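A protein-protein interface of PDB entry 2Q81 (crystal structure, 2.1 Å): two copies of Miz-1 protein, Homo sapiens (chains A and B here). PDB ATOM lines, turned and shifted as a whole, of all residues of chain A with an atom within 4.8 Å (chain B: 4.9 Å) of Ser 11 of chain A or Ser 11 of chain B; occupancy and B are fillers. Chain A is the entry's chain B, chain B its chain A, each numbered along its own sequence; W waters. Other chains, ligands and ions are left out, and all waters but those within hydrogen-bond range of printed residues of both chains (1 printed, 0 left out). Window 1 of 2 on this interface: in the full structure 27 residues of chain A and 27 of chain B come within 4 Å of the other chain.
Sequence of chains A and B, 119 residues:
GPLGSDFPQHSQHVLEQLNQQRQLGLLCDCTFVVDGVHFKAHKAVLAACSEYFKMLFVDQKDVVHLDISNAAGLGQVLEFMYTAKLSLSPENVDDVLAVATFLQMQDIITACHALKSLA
Phe 7 of chain A touches Gln 12 of chain B, and with the chains exchanged Gln 12 of chain A touches Phe 7 of chain B. Pro 8 of chain A touches Gln 12 of chain B, and with the chains exchanged Gln 12 of chain A touches Pro 8 of chain B. Ser 11 of chain A touches Gln 12 of chain B, and with the chains exchanged Gln 12 of chain A touches Ser 11 of chain B. Ser 11 of chain A touches Leu 15 of chain B, and with the chains exchanged Leu 15 of chain A touches Ser 11 of chain B. Positions printed for both chains: 7, 8, 9, 10, 11, 12, 13, 14 and 15.
Of the 10 printed residues of chain B, 5 touch a printed residue of chain A. Hydrophobic or aromatic side chains of chain B that line the printed part of chain A: Phe 7, Pro 8 and Leu 15. Among the printed residues, 12 pairs touch across the chains. Among the printed residues, no Asp or Glu carboxylate lies within 4 Å of a Lys or Arg side-chain nitrogen of the other chain.
Of the printed residues of chain B, Ser 11 of chain A touches Ser 11 (3.5 Å), Gln 12 (3.2 Å) and Leu 15 (3.8 Å). Printed residues of chain A within 4 Å of Ser 11 of chain B: Ser 11, Gln 12 and Leu 15. Of the printed residues of chain A, Leu 15 of chain B touches Phe 7 (3.7 Å), His 10 (3.5 Å) and Ser 11 (3.8 Å). Of the printed residues of chain B, Phe 7 of chain A touches Gln 12 and Leu 15. His 13 of chain A touches none of the printed residues of chain B. The nearest printed residue of chain B that does not touch Ser 11 of chain A is Pro 8 of chain B (4.1 Å). The nearest printed residue of chain A that does not touch Ser 11 of chain B is Pro 8 of chain A (5.5 Å).
Among the printed residues, pairs that only touch across the chains: Phe 7 of chain A with Gln 12 of chain B, Phe 7 of chain A with Leu 15 of chain B, Pro 8 of chain A with Gln 12 of chain B, His 10 of chain A with Leu 15 of chain B, Ser 11 of chain A with Ser 11 of chain B, Ser 11 of chain A with Leu 15 of chain B, Gln 12 of chain A with Phe 7 of chain B, Gln 12 of chain A with Pro 8 of chain B, Gln 12 of chain A with Ser 11 of chain B, Leu 15 of chain A with Phe 7 of chain B and Leu 15 of chain A with Ser 11 of chain B.
The backbone NH (N) of Gln 12 of chain B sits close to the side-chain hydroxyl (OG) of Ser 11 of chain A (3.3 Å).
Water W1 bridges the backbone carbonyl oxygen (O) of Ser 11 of chain B (3.4 Å) and the backbone carbonyl oxygen (O) of Ser 11 of chain A (3.5 Å).
The backbone carbonyl oxygen (O) of Phe 7 of chain B sits at hydrogen-bond distance from the side-chain hydroxyl (OG) of Ser 11 of chain B. The side-chain amide oxygen (OE1) of Gln 12 of chain B lies close to the backbone carbonyl oxygen (O) of Pro 8 of chain B, 3.2 Å away. OG of Ser 11 of chain A lies within hydrogen-bond range of O of Pro 8 of chain A, 3.0 Å away. O of Phe 7 of chain A sits at hydrogen-bond distance from OG of Ser 11 of chain A, 3.2 Å away. The side-chain amide nitrogen (NE2) of Gln 12 of chain A lies close to the backbone carbonyl oxygen (O) of Pro 8 of chain A (3.3 Å).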
ATOM      1  N   PHE A   7      -7.481 -13.465 -13.544  1.00  0.00           N
ATOM      2  CA  PHE A   7      -7.768 -14.495 -12.542  1.00  0.00           C
ATOM      3  C   PHE A   7      -9.129 -14.309 -11.840  1.00  0.00           C
ATOM      4  O   PHE A   7      -9.841 -15.292 -11.660  1.00  0.00           O
ATOM      5  CB  PHE A   7      -6.621 -14.645 -11.524  1.00  0.00           C
ATOM      6  CG  PHE A   7      -6.812 -15.783 -10.550  1.00  0.00           C
ATOM      7  CD1 PHE A   7      -6.652 -17.109 -10.961  1.00  0.00           C
ATOM      8  CD2 PHE A   7      -7.150 -15.529  -9.223  1.00  0.00           C
ATOM      9  CE1 PHE A   7      -6.830 -18.157 -10.065  1.00  0.00           C
ATOM     10  CE2 PHE A   7      -7.332 -16.566  -8.315  1.00  0.00           C
ATOM     11  CZ  PHE A   7      -7.176 -17.888  -8.730  1.00  0.00           C
ATOM     12  N   PRO A   8      -9.491 -13.062 -11.442  1.00  0.00           N
ATOM     13  CA  PRO A   8     -10.842 -12.863 -10.916  1.00  0.00           C
ATOM     14  C   PRO A   8     -11.954 -13.383 -11.847  1.00  0.00           C
ATOM     15  O   PRO A   8     -12.749 -14.211 -11.414  1.00  0.00           O
ATOM     16  CB  PRO A   8     -10.932 -11.336 -10.745  1.00  0.00           C
ATOM     17  CG  PRO A   8      -9.520 -10.916 -10.513  1.00  0.00           C
ATOM     18  CD  PRO A   8      -8.706 -11.809 -11.397  1.00  0.00           C
ATOM     19  N   GLN A   9     -11.992 -12.910 -13.101  1.00  0.00           N
ATOM     20  CA  GLN A   9     -12.982 -13.361 -14.097  1.00  0.00           C
ATOM     21  C   GLN A   9     -12.857 -14.877 -14.359  1.00  0.00           C
ATOM     22  O   GLN A   9     -13.857 -15.595 -14.470  1.00  0.00           O
ATOM     23  CB  GLN A   9     -12.837 -12.582 -15.418  1.00  0.00           C
ATOM     24  CG  GLN A   9     -13.243 -11.085 -15.356  1.00  0.00           C
ATOM     25  CD  GLN A   9     -12.846 -10.291 -16.613  1.00  0.00           C
ATOM     26  OE1 GLN A   9     -12.636 -10.859 -17.695  1.00  0.00           O
ATOM     27  NE2 GLN A   9     -12.748  -8.970 -16.471  1.00  0.00           N
ATOM     28  N   HIS A  10     -11.618 -15.344 -14.445  1.00  0.00           N
ATOM     29  CA  HIS A  10     -11.326 -16.735 -14.712  1.00  0.00           C
ATOM     30  C   HIS A  10     -11.864 -17.657 -13.602  1.00  0.00           C
ATOM     31  O   HIS A  10     -12.519 -18.653 -13.898  1.00  0.00           O
ATOM     32  CB  HIS A  10      -9.826 -16.904 -14.931  1.00  0.00           C
ATOM     33  CG  HIS A  10      -9.411 -18.300 -15.251  1.00  0.00           C
ATOM     34  ND1 HIS A  10      -9.178 -18.731 -16.539  1.00  0.00           N
ATOM     35  CD2 HIS A  10      -9.166 -19.360 -14.447  1.00  0.00           C
ATOM     36  CE1 HIS A  10      -8.824 -20.003 -16.516  1.00  0.00           C
ATOM     37  NE2 HIS A  10      -8.814 -20.410 -15.257  1.00  0.00           N
ATOM     38  N   SER A  11     -11.620 -17.306 -12.335  1.00  0.00           N
ATOM     39  CA  SER A  11     -12.093 -18.123 -11.211  1.00  0.00           C
ATOM     40  C   SER A  11     -13.616 -18.144 -11.124  1.00  0.00           C
ATOM     41  O   SER A  11     -14.203 -19.175 -10.812  1.00  0.00           O
ATOM     42  CB  SER A  11     -11.503 -17.649  -9.878  1.00  0.00           C
ATOM     43  OG  SER A  11     -11.956 -16.351  -9.534  1.00  0.00           O
ATOM     44  N   GLN A  12     -14.252 -17.002 -11.394  1.00  0.00           N
ATOM     45  CA  GLN A  12     -15.714 -16.937 -11.408  1.00  0.00           C
ATOM     46  C   GLN A  12     -16.309 -17.901 -12.433  1.00  0.00           C
ATOM     47  O   GLN A  12     -17.273 -18.601 -12.123  1.00  0.00           O
ATOM     48  CB  GLN A  12     -16.205 -15.505 -11.635  1.00  0.00           C
ATOM     49  CG  GLN A  12     -15.818 -14.559 -10.491  1.00  0.00           C
ATOM     50  CD  GLN A  12     -16.269 -13.145 -10.728  1.00  0.00           C
ATOM     51  OE1 GLN A  12     -17.468 -12.853 -10.689  1.00  0.00           O
ATOM     52  NE2 GLN A  12     -15.316 -12.247 -10.976  1.00  0.00           N
ATOM     53  N   HIS A  13     -15.711 -17.953 -13.629  1.00  0.00           N
ATOM     54  CA  HIS A  13     -16.128 -18.877 -14.687  1.00  0.00           C
ATOM     55  C   HIS A  13     -15.998 -20.325 -14.235  1.00  0.00           C
ATOM     56  O   HIS A  13     -16.937 -21.119 -14.393  1.00  0.00           O
ATOM     57  CB  HIS A  13     -15.314 -18.665 -15.975  1.00  0.00           C
ATOM     58  CG  HIS A  13     -15.516 -19.742 -17.005  1.00  0.00           C
ATOM     59  ND1 HIS A  13     -14.679 -20.834 -17.126  1.00  0.00           N
ATOM     60  CD2 HIS A  13     -16.479 -19.904 -17.945  1.00  0.00           C
ATOM     61  CE1 HIS A  13     -15.110 -21.612 -18.105  1.00  0.00           C
ATOM     62  NE2 HIS A  13     -16.198 -21.066 -18.621  1.00  0.00           N
ATOM     63  N   VAL A  14     -14.833 -20.660 -13.685  1.00  0.00           N
ATOM     64  CA  VAL A  14     -14.567 -22.005 -13.205  1.00  0.00           C
ATOM     65  C   VAL A  14     -15.624 -22.418 -12.171  1.00  0.00           C
ATOM     66  O   VAL A  14     -16.206 -23.487 -12.271  1.00  0.00           O
ATOM     67  CB  VAL A  14     -13.114 -22.153 -12.646  1.00  0.00           C
ATOM     68  CG1 VAL A  14     -12.897 -23.533 -12.031  1.00  0.00           C
ATOM     69  CG2 VAL A  14     -12.066 -21.897 -13.752  1.00  0.00           C
ATOM     70  N   LEU A  15     -15.891 -21.557 -11.197  1.00  0.00           N
ATOM     71  CA  LEU A  15     -16.844 -21.890 -10.140  1.00  0.00           C
ATOM     72  C   LEU A  15     -18.283 -21.997 -10.657  1.00  0.00           C
ATOM     73  O   LEU A  15     -19.046 -22.860 -10.203  1.00  0.00           O
ATOM     74  CB  LEU A  15     -16.746 -20.873  -9.008  1.00  0.00           C
ATOM     75  CG  LEU A  15     -17.286 -21.341  -7.657  1.00  0.00           C
ATOM     76  CD1 LEU A  15     -16.518 -22.525  -7.078  1.00  0.00           C
ATOM     77  CD2 LEU A  15     -17.321 -20.149  -6.659  1.00  0.00           C
ATOM     78  N   ASP B   6     -17.677 -12.049  -1.164  1.00  0.00           N
ATOM     79  CA  ASP B   6     -18.714 -12.264  -2.189  1.00  0.00           C
ATOM     80  C   ASP B   6     -18.151 -13.165  -3.285  1.00  0.00           C
ATOM     81  O   ASP B   6     -17.011 -13.610  -3.186  1.00  0.00           O
ATOM     82  CB  ASP B   6     -19.267 -10.950  -2.758  1.00  0.00           C
ATOM     83  CG  ASP B   6     -20.702 -11.095  -3.299  1.00  0.00           C
ATOM     84  OD1 ASP B   6     -20.874 -11.576  -4.445  1.00  0.00           O
ATOM     85  OD2 ASP B   6     -21.656 -10.714  -2.578  1.00  0.00           O
ATOM     86  N   PHE B   7     -18.949 -13.426  -4.319  1.00  0.00           N
ATOM     87  CA  PHE B   7     -18.600 -14.401  -5.349  1.00  0.00           C
ATOM     88  C   PHE B   7     -17.197 -14.253  -5.969  1.00  0.00           C
ATOM     89  O   PHE B   7     -16.481 -15.245  -6.029  1.00  0.00           O
ATOM     90  CB  PHE B   7     -19.694 -14.500  -6.423  1.00  0.00           C
ATOM     91  CG  PHE B   7     -19.511 -15.661  -7.363  1.00  0.00           C
ATOM     92  CD1 PHE B   7     -19.680 -16.972  -6.917  1.00  0.00           C
ATOM     93  CD2 PHE B   7     -19.158 -15.447  -8.686  1.00  0.00           C
ATOM     94  CE1 PHE B   7     -19.506 -18.051  -7.786  1.00  0.00           C
ATOM     95  CE2 PHE B   7     -18.971 -16.521  -9.561  1.00  0.00           C
ATOM     96  CZ  PHE B   7     -19.146 -17.823  -9.111  1.00  0.00           C
ATOM     97  N   PRO B   8     -16.797 -13.030  -6.417  1.00  0.00           N
ATOM     98  CA  PRO B   8     -15.430 -12.825  -6.941  1.00  0.00           C
ATOM     99  C   PRO B   8     -14.314 -13.305  -6.008  1.00  0.00           C
ATOM    100  O   PRO B   8     -13.491 -14.131  -6.407  1.00  0.00           O
ATOM    101  CB  PRO B   8     -15.343 -11.302  -7.120  1.00  0.00           C
ATOM    102  CG  PRO B   8     -16.749 -10.872  -7.354  1.00  0.00           C
ATOM    103  CD  PRO B   8     -17.589 -11.783  -6.487  1.00  0.00           C
ATOM    104  N   GLN B   9     -14.289 -12.791  -4.782  1.00  0.00           N
ATOM    105  CA  GLN B   9     -13.282 -13.182  -3.800  1.00  0.00           C
ATOM    106  C   GLN B   9     -13.409 -14.662  -3.449  1.00  0.00           C
ATOM    107  O   GLN B   9     -12.414 -15.377  -3.396  1.00  0.00           O
ATOM    108  CB  GLN B   9     -13.398 -12.338  -2.528  1.00  0.00           C
ATOM    109  CG  GLN B   9     -12.884 -10.916  -2.682  1.00  0.00           C
ATOM    110  CD  GLN B   9     -13.293 -10.006  -1.541  1.00  0.00           C
ATOM    111  OE1 GLN B   9     -14.154 -10.351  -0.713  1.00  0.00           O
ATOM    112  NE2 GLN B   9     -12.684  -8.824  -1.493  1.00  0.00           N
ATOM    113  N   HIS B  10     -14.636 -15.117  -3.216  1.00  0.00           N
ATOM    114  CA  HIS B  10     -14.843 -16.496  -2.811  1.00  0.00           C
ATOM    115  C   HIS B  10     -14.416 -17.478  -3.905  1.00  0.00           C
ATOM    116  O   HIS B  10     -13.891 -18.540  -3.605  1.00  0.00           O
ATOM    117  CB  HIS B  10     -16.284 -16.771  -2.386  1.00  0.00           C
ATOM    118  CG  HIS B  10     -16.469 -18.151  -1.834  1.00  0.00           C
ATOM    119  ND1 HIS B  10     -16.664 -19.251  -2.637  1.00  0.00           N
ATOM    120  CD2 HIS B  10     -16.415 -18.616  -0.564  1.00  0.00           C
ATOM    121  CE1 HIS B  10     -16.749 -20.334  -1.887  1.00  0.00           C
ATOM    122  NE2 HIS B  10     -16.599 -19.977  -0.624  1.00  0.00           N
ATOM    123  N   SER B  11     -14.636 -17.116  -5.167  1.00  0.00           N
ATOM    124  CA  SER B  11     -14.252 -17.970  -6.298  1.00  0.00           C
ATOM    125  C   SER B  11     -12.744 -18.034  -6.470  1.00  0.00           C
ATOM    126  O   SER B  11     -12.197 -19.092  -6.781  1.00  0.00           O
ATOM    127  CB  SER B  11     -14.898 -17.464  -7.588  1.00  0.00           C
ATOM    128  OG  SER B  11     -16.305 -17.426  -7.409  1.00  0.00           O
ATOM    129  N   GLN B  12     -12.082 -16.893  -6.282  1.00  0.00           N
ATOM    130  CA  GLN B  12     -10.625 -16.822  -6.344  1.00  0.00           C
ATOM    131  C   GLN B  12     -10.013 -17.695  -5.267  1.00  0.00           C
ATOM    132  O   GLN B  12      -9.046 -18.395  -5.525  1.00  0.00           O
ATOM    133  CB  GLN B  12     -10.132 -15.380  -6.193  1.00  0.00           C
ATOM    134  CG  GLN B  12     -10.459 -14.474  -7.385  1.00  0.00           C
ATOM    135  CD  GLN B  12     -10.149 -13.024  -7.113  1.00  0.00           C
ATOM    136  OE1 GLN B  12     -11.048 -12.172  -7.111  1.00  0.00           O
ATOM    137  NE2 GLN B  12      -8.867 -12.725  -6.885  1.00  0.00           N
ATOM    138  N   HIS B  13     -10.585 -17.655  -4.067  1.00  0.00           N
ATOM    139  CA  HIS B  13     -10.116 -18.493  -2.968  1.00  0.00           C
ATOM    140  C   HIS B  13     -10.190 -19.981  -3.332  1.00  0.00           C
ATOM    141  O   HIS B  13      -9.209 -20.703  -3.159  1.00  0.00           O
ATOM    142  CB  HIS B  13     -10.905 -18.225  -1.684  1.00  0.00           C
ATOM    143  CG  HIS B  13     -10.502 -19.104  -0.539  1.00  0.00           C
ATOM    144  ND1 HIS B  13     -11.160 -20.276  -0.228  1.00  0.00           N
ATOM    145  CD2 HIS B  13      -9.507 -18.978   0.371  1.00  0.00           C
ATOM    146  CE1 HIS B  13     -10.590 -20.833   0.825  1.00  0.00           C
ATOM    147  NE2 HIS B  13      -9.586 -20.064   1.209  1.00  0.00           N
ATOM    148  N   VAL B  14     -11.345 -20.416  -3.841  1.00  0.00           N
ATOM    149  CA  VAL B  14     -11.547 -21.819  -4.207  1.00  0.00           C
ATOM    150  C   VAL B  14     -10.579 -22.275  -5.284  1.00  0.00           C
ATOM    151  O   VAL B  14      -9.969 -23.325  -5.139  1.00  0.00           O
ATOM    152  CB  VAL B  14     -13.001 -22.129  -4.639  1.00  0.00           C
ATOM    153  CG1 VAL B  14     -13.118 -23.610  -5.109  1.00  0.00           C
ATOM    154  CG2 VAL B  14     -13.966 -21.847  -3.471  1.00  0.00           C
ATOM    155  N   LEU B  15     -10.417 -21.484  -6.342  1.00  0.00           N
ATOM    156  CA  LEU B  15      -9.487 -21.861  -7.404  1.00  0.00           C
ATOM    157  C   LEU B  15      -8.028 -21.898  -6.931  1.00  0.00           C
ATOM    158  O   LEU B  15      -7.260 -22.741  -7.381  1.00  0.00           O
ATOM    159  CB  LEU B  15      -9.648 -20.979  -8.653  1.00  0.00           C
ATOM    160  CG  LEU B  15      -8.898 -21.498  -9.901  1.00  0.00           C
ATOM    161  CD1 LEU B  15      -9.127 -23.010 -10.146  1.00  0.00           C
ATOM    162  CD2 LEU B  15      -9.247 -20.685 -11.162  1.00  0.00           C
HETATM  163  O   HOH W   1     -13.906 -21.542  -8.306  1.00  0.00           O
